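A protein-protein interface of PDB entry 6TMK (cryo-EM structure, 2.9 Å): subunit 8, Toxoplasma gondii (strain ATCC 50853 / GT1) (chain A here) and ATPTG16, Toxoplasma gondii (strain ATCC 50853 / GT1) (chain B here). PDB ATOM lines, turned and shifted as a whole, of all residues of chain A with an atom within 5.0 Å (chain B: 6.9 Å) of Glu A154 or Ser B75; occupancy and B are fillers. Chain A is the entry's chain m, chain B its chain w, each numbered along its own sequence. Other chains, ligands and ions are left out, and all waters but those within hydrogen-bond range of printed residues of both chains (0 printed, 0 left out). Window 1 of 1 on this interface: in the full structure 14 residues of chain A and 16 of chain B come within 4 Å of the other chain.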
ATOM      1  N   MET A 150     -12.055 -27.015   3.325  1.00  0.00           N
ATOM      2  CA  MET A 150     -11.354 -27.246   2.067  1.00  0.00           C
ATOM      3  C   MET A 150     -11.611 -26.113   1.080  1.00  0.00           C
ATOM      4  O   MET A 150     -10.687 -25.617   0.419  1.00  0.00           O
ATOM      5  CB  MET A 150     -11.800 -28.588   1.497  1.00  0.00           C
ATOM      6  CG  MET A 150     -10.934 -29.149   0.416  1.00  0.00           C
ATOM      7  SD  MET A 150     -10.911 -30.940   0.481  1.00  0.00           S
ATOM      8  CE  MET A 150      -9.748 -31.265  -0.825  1.00  0.00           C
ATOM      9  N   LEU A 151     -12.875 -25.713   0.949  1.00  0.00           N
ATOM     10  CA  LEU A 151     -13.239 -24.611   0.073  1.00  0.00           C
ATOM     11  C   LEU A 151     -12.500 -23.333   0.447  1.00  0.00           C
ATOM     12  O   LEU A 151     -11.997 -22.620  -0.427  1.00  0.00           O
ATOM     13  CB  LEU A 151     -14.746 -24.401   0.144  1.00  0.00           C
ATOM     14  CG  LEU A 151     -15.419 -23.505  -0.884  1.00  0.00           C
ATOM     15  CD1 LEU A 151     -15.517 -24.215  -2.207  1.00  0.00           C
ATOM     16  CD2 LEU A 151     -16.779 -23.124  -0.380  1.00  0.00           C
ATOM     17  N   GLY A 152     -12.427 -23.025   1.741  1.00  0.00           N
ATOM     18  CA  GLY A 152     -11.746 -21.819   2.170  1.00  0.00           C
ATOM     19  C   GLY A 152     -10.255 -21.871   1.910  1.00  0.00           C
ATOM     20  O   GLY A 152      -9.643 -20.867   1.536  1.00  0.00           O
ATOM     21  N   HIS A 153      -9.650 -23.041   2.101  1.00  0.00           N
ATOM     22  CA  HIS A 153      -8.236 -23.203   1.791  1.00  0.00           C
ATOM     23  C   HIS A 153      -7.964 -22.944   0.317  1.00  0.00           C
ATOM     24  O   HIS A 153      -7.046 -22.192  -0.044  1.00  0.00           O
ATOM     25  CB  HIS A 153      -7.777 -24.605   2.168  1.00  0.00           C
ATOM     26  CG  HIS A 153      -6.294 -24.778   2.132  1.00  0.00           C
ATOM     27  ND1 HIS A 153      -5.437 -23.992   2.870  1.00  0.00           N
ATOM     28  CD2 HIS A 153      -5.515 -25.624   1.424  1.00  0.00           C
ATOM     29  CE1 HIS A 153      -4.193 -24.360   2.629  1.00  0.00           C
ATOM     30  NE2 HIS A 153      -4.213 -25.350   1.757  1.00  0.00           N
ATOM     31  N   GLU A 154      -8.754 -23.568  -0.552  1.00  0.00           N
ATOM     32  CA  GLU A 154      -8.549 -23.374  -1.979  1.00  0.00           C
ATOM     33  C   GLU A 154      -8.840 -21.939  -2.396  1.00  0.00           C
ATOM     34  O   GLU A 154      -8.180 -21.418  -3.297  1.00  0.00           O
ATOM     35  CB  GLU A 154      -9.410 -24.355  -2.763  1.00  0.00           C
ATOM     36  CG  GLU A 154      -8.995 -25.798  -2.578  1.00  0.00           C
ATOM     37  CD  GLU A 154      -9.401 -26.685  -3.730  1.00  0.00           C
ATOM     38  OE1 GLU A 154      -9.000 -27.866  -3.737  1.00  0.00           O
ATOM     39  OE2 GLU A 154     -10.122 -26.207  -4.631  1.00  0.00           O
ATOM     40  N   GLY A 155      -9.794 -21.276  -1.741  1.00  0.00           N
ATOM     41  CA  GLY A 155     -10.029 -19.871  -2.024  1.00  0.00           C
ATOM     42  C   GLY A 155      -8.859 -18.995  -1.624  1.00  0.00           C
ATOM     43  O   GLY A 155      -8.509 -18.042  -2.329  1.00  0.00           O
ATOM     44  N   LYS A 156      -8.253 -19.292  -0.477  1.00  0.00           N
ATOM     45  CA  LYS A 156      -7.044 -18.593  -0.061  1.00  0.00           C
ATOM     46  C   LYS A 156      -5.946 -18.738  -1.104  1.00  0.00           C
ATOM     47  O   LYS A 156      -5.286 -17.760  -1.478  1.00  0.00           O
ATOM     48  CB  LYS A 156      -6.583 -19.140   1.283  1.00  0.00           C
ATOM     49  CG  LYS A 156      -5.460 -18.379   1.915  1.00  0.00           C
ATOM     50  CD  LYS A 156      -5.150 -18.902   3.278  1.00  0.00           C
ATOM     51  CE  LYS A 156      -4.359 -20.174   3.200  1.00  0.00           C
ATOM     52  NZ  LYS A 156      -3.828 -20.575   4.526  1.00  0.00           N
ATOM     53  N   ILE A 157      -5.732 -19.964  -1.576  1.00  0.00           N
ATOM     54  CA  ILE A 157      -4.699 -20.198  -2.580  1.00  0.00           C
ATOM     55  C   ILE A 157      -5.027 -19.451  -3.865  1.00  0.00           C
ATOM     56  O   ILE A 157      -4.142 -18.890  -4.524  1.00  0.00           O
ATOM     57  CB  ILE A 157      -4.532 -21.705  -2.832  1.00  0.00           C
ATOM     58  CG1 ILE A 157      -4.056 -22.410  -1.570  1.00  0.00           C
ATOM     59  CG2 ILE A 157      -3.554 -21.946  -3.936  1.00  0.00           C
ATOM     60  CD1 ILE A 157      -4.376 -23.854  -1.547  1.00  0.00           C
ATOM     61  N   HIS A 158      -6.303 -19.442  -4.247  1.00  0.00           N
ATOM     62  CA  HIS A 158      -6.732 -18.727  -5.441  1.00  0.00           C
ATOM     63  C   HIS A 158      -6.399 -17.247  -5.335  1.00  0.00           C
ATOM     64  O   HIS A 158      -5.851 -16.656  -6.268  1.00  0.00           O
ATOM     65  CB  HIS A 158      -8.228 -18.929  -5.654  1.00  0.00           C
ATOM     66  CG  HIS A 158      -8.697 -18.564  -7.025  1.00  0.00           C
ATOM     67  ND1 HIS A 158      -8.502 -17.316  -7.571  1.00  0.00           N
ATOM     68  CD2 HIS A 158      -9.367 -19.281  -7.957  1.00  0.00           C
ATOM     69  CE1 HIS A 158      -9.016 -17.284  -8.786  1.00  0.00           C
ATOM     70  NE2 HIS A 158      -9.550 -18.463  -9.042  1.00  0.00           N
ATOM     71  N   LYS B  73     -17.793 -28.697  -5.420  1.00  0.00           N
ATOM     72  CA  LYS B  73     -16.961 -27.797  -4.628  1.00  0.00           C
ATOM     73  C   LYS B  73     -16.303 -26.758  -5.528  1.00  0.00           C
ATOM     74  O   LYS B  73     -15.100 -26.843  -5.813  1.00  0.00           O
ATOM     75  CB  LYS B  73     -15.911 -28.587  -3.856  1.00  0.00           C
ATOM     76  CG  LYS B  73     -15.244 -27.817  -2.751  1.00  0.00           C
ATOM     77  CD  LYS B  73     -14.025 -28.547  -2.268  1.00  0.00           C
ATOM     78  CE  LYS B  73     -12.844 -28.287  -3.173  1.00  0.00           C
ATOM     79  NZ  LYS B  73     -12.389 -26.889  -3.111  1.00  0.00           N
ATOM     80  N   PRO B  74     -17.051 -25.764  -5.989  1.00  0.00           N
ATOM     81  CA  PRO B  74     -16.438 -24.717  -6.810  1.00  0.00           C
ATOM     82  C   PRO B  74     -15.658 -23.720  -5.971  1.00  0.00           C
ATOM     83  O   PRO B  74     -16.240 -22.856  -5.309  1.00  0.00           O
ATOM     84  CB  PRO B  74     -17.645 -24.066  -7.489  1.00  0.00           C
ATOM     85  CG  PRO B  74     -18.744 -24.253  -6.511  1.00  0.00           C
ATOM     86  CD  PRO B  74     -18.505 -25.584  -5.871  1.00  0.00           C
ATOM     87  N   SER B  75     -14.334 -23.827  -6.012  1.00  0.00           N
ATOM     88  CA  SER B  75     -13.459 -22.882  -5.340  1.00  0.00           C
ATOM     89  C   SER B  75     -13.055 -21.719  -6.229  1.00  0.00           C
ATOM     90  O   SER B  75     -12.586 -20.696  -5.717  1.00  0.00           O
ATOM     91  CB  SER B  75     -12.208 -23.599  -4.842  1.00  0.00           C
ATOM     92  OG  SER B  75     -11.603 -24.341  -5.886  1.00  0.00           O
ATOM     93  N   ASN B  76     -13.219 -21.856  -7.543  1.00  0.00           N
ATOM     94  CA  ASN B  76     -12.934 -20.753  -8.448  1.00  0.00           C
ATOM     95  C   ASN B  76     -13.808 -19.545  -8.145  1.00  0.00           C
ATOM     96  O   ASN B  76     -13.430 -18.410  -8.458  1.00  0.00           O
ATOM     97  CB  ASN B  76     -13.127 -21.212  -9.891  1.00  0.00           C
ATOM     98  CG  ASN B  76     -14.445 -21.918 -10.104  1.00  0.00           C
ATOM     99  OD1 ASN B  76     -15.404 -21.709  -9.365  1.00  0.00           O
ATOM    100  ND2 ASN B  76     -14.494 -22.772 -11.110  1.00  0.00           N
ATOM    101  N   LEU B  77     -14.979 -19.768  -7.553  1.00  0.00           N
ATOM    102  CA  LEU B  77     -15.844 -18.660  -7.176  1.00  0.00           C
ATOM    103  C   LEU B  77     -15.282 -17.874  -6.003  1.00  0.00           C
ATOM    104  O   LEU B  77     -15.571 -16.680  -5.863  1.00  0.00           O
ATOM    105  CB  LEU B  77     -17.226 -19.195  -6.820  1.00  0.00           C
ATOM    106  CG  LEU B  77     -18.001 -19.831  -7.970  1.00  0.00           C
ATOM    107  CD1 LEU B  77     -19.164 -20.644  -7.451  1.00  0.00           C
ATOM    108  CD2 LEU B  77     -18.485 -18.753  -8.898  1.00  0.00           C
ATOM    109  N   LEU B  78     -14.487 -18.515  -5.157  1.00  0.00           N
ATOM    110  CA  LEU B  78     -14.020 -17.917  -3.919  1.00  0.00           C
ATOM    111  C   LEU B  78     -12.559 -17.498  -4.022  1.00  0.00           C
ATOM    112  O   LEU B  78     -11.757 -18.126  -4.715  1.00  0.00           O
ATOM    113  CB  LEU B  78     -14.196 -18.893  -2.756  1.00  0.00           C
ATOM    114  CG  LEU B  78     -14.145 -18.264  -1.370  1.00  0.00           C
ATOM    115  CD1 LEU B  78     -15.402 -17.477  -1.085  1.00  0.00           C
ATOM    116  CD2 LEU B  78     -13.948 -19.335  -0.340  1.00  0.00           C
ATOM    117  N   LYS B  79     -12.222 -16.418  -3.315  1.00  0.00           N
ATOM    118  CA  LYS B  79     -10.856 -15.928  -3.241  1.00  0.00           C
ATOM    119  C   LYS B  79     -10.418 -15.597  -1.824  1.00  0.00           C
ATOM    120  O   LYS B  79      -9.280 -15.159  -1.636  1.00  0.00           O
ATOM    121  CB  LYS B  79     -10.662 -14.691  -4.119  1.00  0.00           C
ATOM    122  CG  LYS B  79     -10.639 -14.989  -5.589  1.00  0.00           C
ATOM    123  CD  LYS B  79     -10.463 -13.741  -6.404  1.00  0.00           C
ATOM    124  CE  LYS B  79     -10.728 -14.016  -7.857  1.00  0.00           C
ATOM    125  NZ  LYS B  79     -10.721 -12.780  -8.661  1.00  0.00           N
ATOM    126  N   ILE B  80     -11.282 -15.775  -0.834  1.00  0.00           N
ATOM    127  CA  ILE B  80     -10.940 -15.511   0.554  1.00  0.00           C
ATOM    128  C   ILE B  80     -10.956 -16.824   1.314  1.00  0.00           C
ATOM    129  O   ILE B  80     -11.664 -17.770   0.956  1.00  0.00           O
ATOM    130  CB  ILE B  80     -11.902 -14.495   1.204  1.00  0.00           C
ATOM    131  CG1 ILE B  80     -13.340 -15.001   1.138  1.00  0.00           C
ATOM    132  CG2 ILE B  80     -11.795 -13.161   0.517  1.00  0.00           C
ATOM    133  CD1 ILE B  80     -14.291 -14.226   1.989  1.00  0.00           C
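The side-chain carboxylate (OE2) of Glu A154 lies within salt-bridge range of the side-chain amino group (NZ) of Lys B73 (2.8 Å). O of Gly A155 sits close to O of Lys B79, at 3.1 Å. OE2 of Glu A154 sits at hydrogen-bond distance from OG of Ser B75.
Among the printed residues, pairs that only touch across the chains: Leu A151 with Lys B73, Leu A151 with Pro B74, Leu A151 with Ser B75, Leu A151 with Leu B78, Gly A152 with Ile B80, Gly A155 with Leu B78, Gly A155 with Ile B80, His A158 with Asn B76, His A158 with Leu B78 and His A158 with Lys B79.
Glu A154 touches two residues of chain B. Of the printed residues of chain B, His A158 touches Asn B76, Leu B78 and Lys B79. Of the printed residues of chain A, Ile B80 touches Gly A152 (3.7 Å) and Gly A155 (3.9 Å). The nearest residue of chain A that does not touch Ser B75 is His A158 (4.2 Å). The nearest printed residue of chain A that does not touch Leu B78 is Gly A152 (4.2 Å).
Printed residues of chain B that touch a printed residue of chain A: Lys B73, Pro B74, Ser B75, Asn B76, Leu B78, Lys B79 and Ile B80. Hydrophobic or aromatic side chains of chain B that line the printed part of chain A: Leu B78. Of the 9 printed residues of chain A, 5 touch a printed residue of chain B. Printed residues of chain A that touch a printed residue of chain B: Leu A151, Gly A152, Glu A154, Gly A155 and His A158. Among the printed residues, 13 pairs touch across the chains. Among the printed residues, Asp or Glu carboxylates within 4 Å of a Lys or Arg side-chain nitrogen of the other chain: Glu A154 with Lys B73 (2.8 Å).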
